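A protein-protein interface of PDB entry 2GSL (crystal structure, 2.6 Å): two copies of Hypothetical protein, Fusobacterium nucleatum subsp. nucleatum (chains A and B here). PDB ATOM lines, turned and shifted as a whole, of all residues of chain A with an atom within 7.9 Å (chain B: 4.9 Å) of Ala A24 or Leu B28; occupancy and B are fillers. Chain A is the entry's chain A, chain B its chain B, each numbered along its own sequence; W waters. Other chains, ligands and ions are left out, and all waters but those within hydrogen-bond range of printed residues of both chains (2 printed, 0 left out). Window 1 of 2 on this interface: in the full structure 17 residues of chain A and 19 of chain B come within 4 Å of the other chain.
NH1 of Arg B31 sits at hydrogen-bond distance from O of Phe A20 (3.0 Å).
NH1 of Arg B31 lies within salt-bridge range of OD2 of Asp A23 (3.1 Å).
OH of Tyr A110 lies within hydrogen-bond range of NZ of Lys B32 (2.7 Å).
The guanidinium group (NH1) of Arg B31 lies close to the backbone NH (N) of Ala A24.
Water W2 bridges the backbone carbonyl oxygen (O) of Ala A24 (2.6 Å) and the backbone carbonyl oxygen (O) of Ala B24 (2.7 Å).
Water W1 lies within hydrogen-bond range of the guanidinium group (NH2) of Arg B31 (2.9 Å) and the side-chain carboxylate (OD2) of Asp A23 (3.1 Å).
Ala A24 touches two residues of chain B.
Printed residues of chain B within 4 Å of Leu A28: Ala B24 (3.9 Å), Ile B25 (3.6 Å) and Leu B28 (3.8 Å).
Of the printed residues of chain B, Tyr A110 touches Leu B28 and Lys B32.
Printed residues of chain A within 4 Å of Ala B24: Leu A28 and Arg A31.
Leu B28 touches just these residues of chain A: Leu A21 (3.5 Å), Ala A24 (3.8 Å), Ile A25 (3.5 Å), Leu A28 (3.8 Å) and Tyr A110 (3.9 Å).
Printed residues of chain A within 4 Å of Lys B32: Leu A21 (3.6 Å) and Tyr A110 (2.7 Å).
The nearest residue of chain B that does not touch Ala A24 is Glu B27 (4.7 Å).
NH2 of Arg A31 is in salt-bridge range of OE2 of Glu A27.
NE of Arg B31 is in salt-bridge range of OE2 of Glu B27 (2.4 Å).
The side-chain amino group (NZ) of Lys B32 is in salt-bridge range of the side-chain carboxylate (OE1) of Glu B29 (3.3 Å).
Ala A24 touches Leu B28, and with the chains exchanged Leu A28 touches Ala B24.
Ala A24 touches Arg B31, and with the chains exchanged Arg A31 touches Ala B24.
Ile A25 touches Leu B28, and with the chains exchanged Leu A28 touches Ile B25.
Leu A28 touches its own counterpart, Leu B28.
Positions printed for both chains: 24, 25, 26, 27, 28, 29, 30 and 31.
Of the 13 pairs that touch across the chains among the printed residues, 7 have their exchanged pair printed and touching as well.
Leu A21 touches Leu B28.
Lys B32 touches Leu A21 (CG to CD1, 3.6 Å).
Leu B28 touches Ala A24.
Ile A25 touches Leu B28.
Leu A28 touches Ala B24 (CD1 to CB, 3.9 Å).
Leu A28 touches Ile B25 (CD1 to CG1, 3.6 Å).
Leu A28 touches Leu B28 (CD2 to CD2, 3.8 Å).
Arg A31 touches Ala B24.
Tyr A110 touches Leu B28 (OH to CD2, 3.9 Å).
Printed residues of chain A that touch a printed residue of chain B: Phe A20, Leu A21, Asp A23, Ala A24, Ile A25, Leu A28, Arg A31 and Tyr A110.
Hydrophobic or aromatic side chains of chain A within 4 Å of the printed part of chain B: Phe A20, Leu A21, Ala A24, Ile A25, Leu A28 and Tyr A110.
Among the printed residues, 13 pairs touch across the chains.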
ATOM      1  N   LEU A  18      -2.257 -14.139 -15.204  1.00  0.00           N
ATOM      2  CA  LEU A  18      -2.203 -13.821 -13.790  1.00  0.00           C
ATOM      3  C   LEU A  18      -1.889 -15.086 -13.003  1.00  0.00           C
ATOM      4  O   LEU A  18      -1.011 -15.093 -12.143  1.00  0.00           O
ATOM      5  CB  LEU A  18      -3.539 -13.231 -13.328  1.00  0.00           C
ATOM      6  CG  LEU A  18      -3.986 -11.941 -14.031  1.00  0.00           C
ATOM      7  CD1 LEU A  18      -5.453 -11.706 -13.734  1.00  0.00           C
ATOM      8  CD2 LEU A  18      -3.134 -10.748 -13.568  1.00  0.00           C
ATOM      9  N   ALA A  19      -2.609 -16.157 -13.305  1.00  0.00           N
ATOM     10  CA  ALA A  19      -2.415 -17.438 -12.626  1.00  0.00           C
ATOM     11  C   ALA A  19      -0.964 -17.911 -12.730  1.00  0.00           C
ATOM     12  O   ALA A  19      -0.474 -18.643 -11.870  1.00  0.00           O
ATOM     13  CB  ALA A  19      -3.346 -18.489 -13.234  1.00  0.00           C
ATOM     14  N   PHE A  20      -0.295 -17.496 -13.802  1.00  0.00           N
ATOM     15  CA  PHE A  20       1.097 -17.856 -14.051  1.00  0.00           C
ATOM     16  C   PHE A  20       1.965 -17.133 -13.032  1.00  0.00           C
ATOM     17  O   PHE A  20       2.868 -17.712 -12.422  1.00  0.00           O
ATOM     18  CB  PHE A  20       1.495 -17.438 -15.475  1.00  0.00           C
ATOM     19  CG  PHE A  20       2.864 -17.909 -15.898  1.00  0.00           C
ATOM     20  CD1 PHE A  20       3.233 -19.249 -15.757  1.00  0.00           C
ATOM     21  CD2 PHE A  20       3.773 -17.022 -16.480  1.00  0.00           C
ATOM     22  CE1 PHE A  20       4.484 -19.693 -16.192  1.00  0.00           C
ATOM     23  CE2 PHE A  20       5.017 -17.461 -16.916  1.00  0.00           C
ATOM     24  CZ  PHE A  20       5.380 -18.796 -16.775  1.00  0.00           C
ATOM     25  N   LEU A  21       1.681 -15.851 -12.863  1.00  0.00           N
ATOM     26  CA  LEU A  21       2.403 -15.030 -11.922  1.00  0.00           C
ATOM     27  C   LEU A  21       1.985 -15.465 -10.517  1.00  0.00           C
ATOM     28  O   LEU A  21       2.830 -15.690  -9.651  1.00  0.00           O
ATOM     29  CB  LEU A  21       2.059 -13.554 -12.164  1.00  0.00           C
ATOM     30  CG  LEU A  21       2.475 -12.550 -11.092  1.00  0.00           C
ATOM     31  CD1 LEU A  21       3.984 -12.515 -10.988  1.00  0.00           C
ATOM     32  CD2 LEU A  21       1.922 -11.189 -11.437  1.00  0.00           C
ATOM     33  N   GLY A  22       0.675 -15.595 -10.309  1.00  0.00           N
ATOM     34  CA  GLY A  22       0.156 -16.009  -9.013  1.00  0.00           C
ATOM     35  C   GLY A  22       0.788 -17.283  -8.480  1.00  0.00           C
ATOM     36  O   GLY A  22       1.052 -17.396  -7.290  1.00  0.00           O
ATOM     37  N   ASP A  23       1.026 -18.239  -9.373  1.00  0.00           N
ATOM     38  CA  ASP A  23       1.629 -19.524  -9.032  1.00  0.00           C
ATOM     39  C   ASP A  23       2.997 -19.322  -8.380  1.00  0.00           C
ATOM     40  O   ASP A  23       3.272 -19.885  -7.314  1.00  0.00           O
ATOM     41  CB  ASP A  23       1.758 -20.381 -10.304  1.00  0.00           C
ATOM     42  CG  ASP A  23       2.464 -21.714 -10.059  1.00  0.00           C
ATOM     43  OD1 ASP A  23       1.935 -22.526  -9.278  1.00  0.00           O
ATOM     44  OD2 ASP A  23       3.538 -21.943 -10.658  1.00  0.00           O
ATOM     45  N   ALA A  24       3.845 -18.521  -9.026  1.00  0.00           N
ATOM     46  CA  ALA A  24       5.179 -18.221  -8.512  1.00  0.00           C
ATOM     47  C   ALA A  24       5.086 -17.495  -7.173  1.00  0.00           C
ATOM     48  O   ALA A  24       5.892 -17.739  -6.261  1.00  0.00           O
ATOM     49  CB  ALA A  24       5.955 -17.372  -9.516  1.00  0.00           C
ATOM     50  N   ILE A  25       4.091 -16.617  -7.050  1.00  0.00           N
ATOM     51  CA  ILE A  25       3.886 -15.838  -5.826  1.00  0.00           C
ATOM     52  C   ILE A  25       3.498 -16.771  -4.683  1.00  0.00           C
ATOM     53  O   ILE A  25       3.953 -16.607  -3.542  1.00  0.00           O
ATOM     54  CB  ILE A  25       2.763 -14.763  -6.026  1.00  0.00           C
ATOM     55  CG1 ILE A  25       3.176 -13.771  -7.120  1.00  0.00           C
ATOM     56  CG2 ILE A  25       2.519 -13.978  -4.750  1.00  0.00           C
ATOM     57  CD1 ILE A  25       2.076 -12.835  -7.528  1.00  0.00           C
ATOM     58  N   TRP A  26       2.647 -17.747  -5.002  1.00  0.00           N
ATOM     59  CA  TRP A  26       2.170 -18.723  -4.019  1.00  0.00           C
ATOM     60  C   TRP A  26       3.333 -19.576  -3.539  1.00  0.00           C
ATOM     61  O   TRP A  26       3.533 -19.713  -2.327  1.00  0.00           O
ATOM     62  CB  TRP A  26       1.089 -19.620  -4.637  1.00  0.00           C
ATOM     63  CG  TRP A  26       0.348 -20.453  -3.656  1.00  0.00           C
ATOM     64  CD1 TRP A  26       0.508 -21.781  -3.431  1.00  0.00           C
ATOM     65  CD2 TRP A  26      -0.693 -20.017  -2.772  1.00  0.00           C
ATOM     66  NE1 TRP A  26      -0.366 -22.204  -2.454  1.00  0.00           N
ATOM     67  CE2 TRP A  26      -1.105 -21.135  -2.029  1.00  0.00           C
ATOM     68  CE3 TRP A  26      -1.297 -18.782  -2.520  1.00  0.00           C
ATOM     69  CZ2 TRP A  26      -2.118 -21.063  -1.077  1.00  0.00           C
ATOM     70  CZ3 TRP A  26      -2.304 -18.707  -1.570  1.00  0.00           C
ATOM     71  CH2 TRP A  26      -2.696 -19.834  -0.854  1.00  0.00           C
ATOM     72  N   GLU A  27       4.111 -20.134  -4.466  1.00  0.00           N
ATOM     73  CA  GLU A  27       5.242 -20.963  -4.042  1.00  0.00           C
ATOM     74  C   GLU A  27       6.096 -20.186  -3.058  1.00  0.00           C
ATOM     75  O   GLU A  27       6.305 -20.628  -1.928  1.00  0.00           O
ATOM     76  CB  GLU A  27       6.105 -21.427  -5.232  1.00  0.00           C
ATOM     77  CG  GLU A  27       5.825 -22.863  -5.682  1.00  0.00           C
ATOM     78  CD  GLU A  27       6.790 -23.901  -5.099  1.00  0.00           C
ATOM     79  OE1 GLU A  27       6.886 -24.044  -3.866  1.00  0.00           O
ATOM     80  OE2 GLU A  27       7.465 -24.606  -5.877  1.00  0.00           O
ATOM     81  N   LEU A  28       6.564 -19.013  -3.481  1.00  0.00           N
ATOM     82  CA  LEU A  28       7.421 -18.161  -2.645  1.00  0.00           C
ATOM     83  C   LEU A  28       6.936 -18.028  -1.212  1.00  0.00           C
ATOM     84  O   LEU A  28       7.681 -18.304  -0.280  1.00  0.00           O
ATOM     85  CB  LEU A  28       7.545 -16.764  -3.259  1.00  0.00           C
ATOM     86  CG  LEU A  28       8.483 -15.815  -2.533  1.00  0.00           C
ATOM     87  CD1 LEU A  28       9.824 -16.508  -2.299  1.00  0.00           C
ATOM     88  CD2 LEU A  28       8.661 -14.572  -3.355  1.00  0.00           C
ATOM     89  N   GLU A  29       5.695 -17.595  -1.041  1.00  0.00           N
ATOM     90  CA  GLU A  29       5.141 -17.439   0.283  1.00  0.00           C
ATOM     91  C   GLU A  29       5.154 -18.759   1.053  1.00  0.00           C
ATOM     92  O   GLU A  29       5.543 -18.783   2.222  1.00  0.00           O
ATOM     93  CB  GLU A  29       3.726 -16.879   0.193  1.00  0.00           C
ATOM     94  CG  GLU A  29       3.698 -15.419  -0.214  1.00  0.00           C
ATOM     95  CD  GLU A  29       4.662 -14.566   0.611  1.00  0.00           C
ATOM     96  OE1 GLU A  29       5.631 -14.012   0.030  1.00  0.00           O
ATOM     97  OE2 GLU A  29       4.445 -14.464   1.839  1.00  0.00           O
ATOM     98  N   ILE A  30       4.754 -19.859   0.408  1.00  0.00           N
ATOM     99  CA  ILE A  30       4.736 -21.162   1.085  1.00  0.00           C
ATOM    100  C   ILE A  30       6.143 -21.610   1.481  1.00  0.00           C
ATOM    101  O   ILE A  30       6.365 -22.039   2.612  1.00  0.00           O
ATOM    102  CB  ILE A  30       4.057 -22.265   0.213  1.00  0.00           C
ATOM    103  CG1 ILE A  30       2.572 -21.942   0.042  1.00  0.00           C
ATOM    104  CG2 ILE A  30       4.179 -23.623   0.875  1.00  0.00           C
ATOM    105  CD1 ILE A  30       1.842 -21.675   1.343  1.00  0.00           C
ATOM    106  N   ARG A  31       7.104 -21.503   0.574  1.00  0.00           N
ATOM    107  CA  ARG A  31       8.444 -21.923   0.939  1.00  0.00           C
ATOM    108  C   ARG A  31       8.970 -21.067   2.083  1.00  0.00           C
ATOM    109  O   ARG A  31       9.617 -21.580   3.007  1.00  0.00           O
ATOM    110  CB  ARG A  31       9.371 -21.834  -0.252  1.00  0.00           C
ATOM    111  CG  ARG A  31       8.934 -22.719  -1.382  1.00  0.00           C
ATOM    112  CD  ARG A  31      10.035 -22.785  -2.382  1.00  0.00           C
ATOM    113  NE  ARG A  31       9.708 -23.614  -3.525  1.00  0.00           N
ATOM    114  CZ  ARG A  31      10.536 -23.806  -4.548  1.00  0.00           C
ATOM    115  NH1 ARG A  31      11.732 -23.222  -4.543  1.00  0.00           N
ATOM    116  NH2 ARG A  31      10.174 -24.567  -5.581  1.00  0.00           N
ATOM    117  N   VAL A  52       0.760 -26.520  -2.085  1.00  0.00           N
ATOM    118  CA  VAL A  52       1.018 -25.926  -3.376  1.00  0.00           C
ATOM    119  C   VAL A  52       0.218 -26.620  -4.504  1.00  0.00           C
ATOM    120  O   VAL A  52       0.197 -26.140  -5.638  1.00  0.00           O
ATOM    121  CB  VAL A  52       2.542 -25.990  -3.653  1.00  0.00           C
ATOM    122  CG1 VAL A  52       2.835 -26.857  -4.864  1.00  0.00           C
ATOM    123  CG2 VAL A  52       3.106 -24.592  -3.813  1.00  0.00           C
ATOM    124  N   GLU A 103      -4.882 -18.669  -8.119  1.00  0.00           N
ATOM    125  CA  GLU A 103      -3.589 -18.105  -8.510  1.00  0.00           C
ATOM    126  C   GLU A 103      -3.770 -16.844  -9.354  1.00  0.00           C
ATOM    127  O   GLU A 103      -2.848 -16.041  -9.496  1.00  0.00           O
ATOM    128  CB  GLU A 103      -2.752 -19.122  -9.302  1.00  0.00           C
ATOM    129  CG  GLU A 103      -2.502 -20.422  -8.582  1.00  0.00           C
ATOM    130  CD  GLU A 103      -1.474 -21.293  -9.265  1.00  0.00           C
ATOM    131  OE1 GLU A 103      -0.536 -21.737  -8.561  1.00  0.00           O
ATOM    132  OE2 GLU A 103      -1.588 -21.548 -10.493  1.00  0.00           O
ATOM    133  N   ILE A 106      -4.434 -14.084  -6.635  1.00  0.00           N
ATOM    134  CA  ILE A 106      -3.168 -13.794  -5.978  1.00  0.00           C
ATOM    135  C   ILE A 106      -2.308 -12.984  -6.949  1.00  0.00           C
ATOM    136  O   ILE A 106      -1.722 -11.971  -6.577  1.00  0.00           O
ATOM    137  CB  ILE A 106      -2.389 -15.113  -5.556  1.00  0.00           C
ATOM    138  CG1 ILE A 106      -3.141 -15.868  -4.461  1.00  0.00           C
ATOM    139  CG2 ILE A 106      -1.018 -14.763  -4.969  1.00  0.00           C
ATOM    140  CD1 ILE A 106      -3.118 -15.164  -3.105  1.00  0.00           C
ATOM    141  N   GLY A 107      -2.236 -13.431  -8.197  1.00  0.00           N
ATOM    142  CA  GLY A 107      -1.439 -12.722  -9.179  1.00  0.00           C
ATOM    143  C   GLY A 107      -1.886 -11.282  -9.340  1.00  0.00           C
ATOM    144  O   GLY A 107      -1.057 -10.374  -9.462  1.00  0.00           O
ATOM    145  N   TYR A 110      -1.060  -8.827  -6.319  1.00  0.00           N
ATOM    146  CA  TYR A 110       0.329  -8.418  -6.379  1.00  0.00           C
ATOM    147  C   TYR A 110       0.485  -7.215  -7.324  1.00  0.00           C
ATOM    148  O   TYR A 110       0.899  -6.136  -6.903  1.00  0.00           O
ATOM    149  CB  TYR A 110       1.163  -9.591  -6.861  1.00  0.00           C
ATOM    150  CG  TYR A 110       2.635  -9.405  -6.682  1.00  0.00           C
ATOM    151  CD1 TYR A 110       3.262  -9.753  -5.501  1.00  0.00           C
ATOM    152  CD2 TYR A 110       3.410  -8.925  -7.723  1.00  0.00           C
ATOM    153  CE1 TYR A 110       4.631  -9.636  -5.369  1.00  0.00           C
ATOM    154  CE2 TYR A 110       4.769  -8.802  -7.606  1.00  0.00           C
ATOM    155  CZ  TYR A 110       5.379  -9.162  -6.434  1.00  0.00           C
ATOM    156  OH  TYR A 110       6.749  -9.079  -6.358  1.00  0.00           O
ATOM    157  N   GLU A 115      -0.215  -6.339  -1.775  1.00  0.00           N
ATOM    158  CA  GLU A 115       0.520  -7.410  -1.121  1.00  0.00           C
ATOM    159  C   GLU A 115       0.036  -7.639   0.311  1.00  0.00           C
ATOM    160  O   GLU A 115       0.361  -8.652   0.931  1.00  0.00           O
ATOM    161  CB  GLU A 115       2.030  -7.106  -1.134  1.00  0.00           C
ATOM    162  CG  GLU A 115       2.897  -8.095  -1.946  1.00  0.00           C
ATOM    163  CD  GLU A 115       3.428  -9.264  -1.102  1.00  0.00           C
ATOM    164  OE1 GLU A 115       4.212  -9.013  -0.159  1.00  0.00           O
ATOM    165  OE2 GLU A 115       3.064 -10.432  -1.378  1.00  0.00           O
ATOM    166  N   ALA B  24      12.778 -19.641  -5.839  1.00  0.00           N
ATOM    167  CA  ALA B  24      11.421 -19.183  -5.973  1.00  0.00           C
ATOM    168  C   ALA B  24      11.403 -17.685  -6.282  1.00  0.00           C
ATOM    169  O   ALA B  24      10.612 -17.230  -7.117  1.00  0.00           O
ATOM    170  CB  ALA B  24      10.636 -19.506  -4.708  1.00  0.00           C
ATOM    171  N   ILE B  25      12.277 -16.925  -5.621  1.00  0.00           N
ATOM    172  CA  ILE B  25      12.384 -15.469  -5.819  1.00  0.00           C
ATOM    173  C   ILE B  25      12.756 -15.215  -7.280  1.00  0.00           C
ATOM    174  O   ILE B  25      12.063 -14.501  -8.013  1.00  0.00           O
ATOM    175  CB  ILE B  25      13.455 -14.879  -4.828  1.00  0.00           C
ATOM    176  CG1 ILE B  25      12.876 -14.916  -3.409  1.00  0.00           C
ATOM    177  CG2 ILE B  25      13.843 -13.443  -5.198  1.00  0.00           C
ATOM    178  CD1 ILE B  25      13.895 -14.918  -2.313  1.00  0.00           C
ATOM    179  N   TRP B  26      13.842 -15.833  -7.712  1.00  0.00           N
ATOM    180  CA  TRP B  26      14.271 -15.694  -9.091  1.00  0.00           C
ATOM    181  C   TRP B  26      13.121 -15.972 -10.065  1.00  0.00           C
ATOM    182  O   TRP B  26      12.834 -15.146 -10.930  1.00  0.00           O
ATOM    183  CB  TRP B  26      15.431 -16.641  -9.362  1.00  0.00           C
ATOM    184  CG  TRP B  26      16.042 -16.473 -10.684  1.00  0.00           C
ATOM    185  CD1 TRP B  26      15.748 -17.172 -11.808  1.00  0.00           C
ATOM    186  CD2 TRP B  26      17.110 -15.580 -11.026  1.00  0.00           C
ATOM    187  NE1 TRP B  26      16.574 -16.780 -12.836  1.00  0.00           N
ATOM    188  CE2 TRP B  26      17.420 -15.801 -12.380  1.00  0.00           C
ATOM    189  CE3 TRP B  26      17.832 -14.611 -10.315  1.00  0.00           C
ATOM    190  CZ2 TRP B  26      18.428 -15.097 -13.041  1.00  0.00           C
ATOM    191  CZ3 TRP B  26      18.835 -13.909 -10.968  1.00  0.00           C
ATOM    192  CH2 TRP B  26      19.124 -14.154 -12.318  1.00  0.00           C
ATOM    193  N   GLU B  27      12.449 -17.114  -9.933  1.00  0.00           N
ATOM    194  CA  GLU B  27      11.343 -17.412 -10.846  1.00  0.00           C
ATOM    195  C   GLU B  27      10.296 -16.316 -10.883  1.00  0.00           C
ATOM    196  O   GLU B  27       9.838 -15.936 -11.957  1.00  0.00           O
ATOM    197  CB  GLU B  27      10.670 -18.746 -10.496  1.00  0.00           C
ATOM    198  CG  GLU B  27      11.045 -19.873 -11.452  1.00  0.00           C
ATOM    199  CD  GLU B  27      10.022 -20.095 -12.537  1.00  0.00           C
ATOM    200  OE1 GLU B  27      10.356 -20.720 -13.562  1.00  0.00           O
ATOM    201  OE2 GLU B  27       8.869 -19.663 -12.370  1.00  0.00           O
ATOM    202  N   LEU B  28       9.915 -15.809  -9.714  1.00  0.00           N
ATOM    203  CA  LEU B  28       8.908 -14.748  -9.638  1.00  0.00           C
ATOM    204  C   LEU B  28       9.325 -13.520 -10.461  1.00  0.00           C
ATOM    205  O   LEU B  28       8.521 -12.999 -11.234  1.00  0.00           O
ATOM    206  CB  LEU B  28       8.662 -14.341  -8.181  1.00  0.00           C
ATOM    207  CG  LEU B  28       7.613 -13.250  -7.989  1.00  0.00           C
ATOM    208  CD1 LEU B  28       6.305 -13.705  -8.615  1.00  0.00           C
ATOM    209  CD2 LEU B  28       7.423 -12.942  -6.512  1.00  0.00           C
ATOM    210  N   GLU B  29      10.580 -13.081 -10.302  1.00  0.00           N
ATOM    211  CA  GLU B  29      11.102 -11.931 -11.043  1.00  0.00           C
ATOM    212  C   GLU B  29      11.119 -12.217 -12.546  1.00  0.00           C
ATOM    213  O   GLU B  29      10.653 -11.397 -13.343  1.00  0.00           O
ATOM    214  CB  GLU B  29      12.528 -11.566 -10.606  1.00  0.00           C
ATOM    215  CG  GLU B  29      12.707 -11.110  -9.166  1.00  0.00           C
ATOM    216  CD  GLU B  29      11.920  -9.855  -8.818  1.00  0.00           C
ATOM    217  OE1 GLU B  29      10.691  -9.944  -8.622  1.00  0.00           O
ATOM    218  OE2 GLU B  29      12.534  -8.773  -8.749  1.00  0.00           O
ATOM    219  N   ILE B  30      11.656 -13.364 -12.951  1.00  0.00           N
ATOM    220  CA  ILE B  30      11.696 -13.651 -14.376  1.00  0.00           C
ATOM    221  C   ILE B  30      10.289 -13.715 -14.931  1.00  0.00           C
ATOM    222  O   ILE B  30      10.034 -13.263 -16.040  1.00  0.00           O
ATOM    223  CB  ILE B  30      12.420 -14.964 -14.693  1.00  0.00           C
ATOM    224  CG1 ILE B  30      13.851 -14.914 -14.164  1.00  0.00           C
ATOM    225  CG2 ILE B  30      12.472 -15.176 -16.186  1.00  0.00           C
ATOM    226  CD1 ILE B  30      14.694 -13.824 -14.771  1.00  0.00           C
ATOM    227  N   ARG B  31       9.357 -14.243 -14.153  1.00  0.00           N
ATOM    228  CA  ARG B  31       7.981 -14.335 -14.625  1.00  0.00           C
ATOM    229  C   ARG B  31       7.319 -12.977 -14.726  1.00  0.00           C
ATOM    230  O   ARG B  31       6.595 -12.710 -15.682  1.00  0.00           O
ATOM    231  CB  ARG B  31       7.167 -15.257 -13.718  1.00  0.00           C
ATOM    232  CG  ARG B  31       7.480 -16.725 -13.966  1.00  0.00           C
ATOM    233  CD  ARG B  31       6.608 -17.578 -13.131  1.00  0.00           C
ATOM    234  NE  ARG B  31       6.789 -18.996 -13.430  1.00  0.00           N
ATOM    235  CZ  ARG B  31       6.076 -19.956 -12.855  1.00  0.00           C
ATOM    236  NH1 ARG B  31       5.141 -19.656 -11.961  1.00  0.00           N
ATOM    237  NH2 ARG B  31       6.302 -21.211 -13.170  1.00  0.00           N
ATOM    238  N   LYS B  32       7.559 -12.122 -13.738  1.00  0.00           N
ATOM    239  CA  LYS B  32       6.990 -10.782 -13.756  1.00  0.00           C
ATOM    240  C   LYS B  32       7.449 -10.019 -14.989  1.00  0.00           C
ATOM    241  O   LYS B  32       6.646  -9.368 -15.655  1.00  0.00           O
ATOM    242  CB  LYS B  32       7.414  -9.994 -12.525  1.00  0.00           C
ATOM    243  CG  LYS B  32       7.011 -10.633 -11.235  1.00  0.00           C
ATOM    244  CD  LYS B  32       6.837  -9.606 -10.135  1.00  0.00           C
ATOM    245  CE  LYS B  32       8.114  -8.858  -9.832  1.00  0.00           C
ATOM    246  NZ  LYS B  32       7.930  -8.117  -8.554  1.00  0.00           N
HETATM  247  O   HOH W   1       5.756 -23.719 -11.887  1.00  0.00           O
HETATM  248  O   HOH W   2       8.183 -18.445  -7.333  1.00  0.00           O
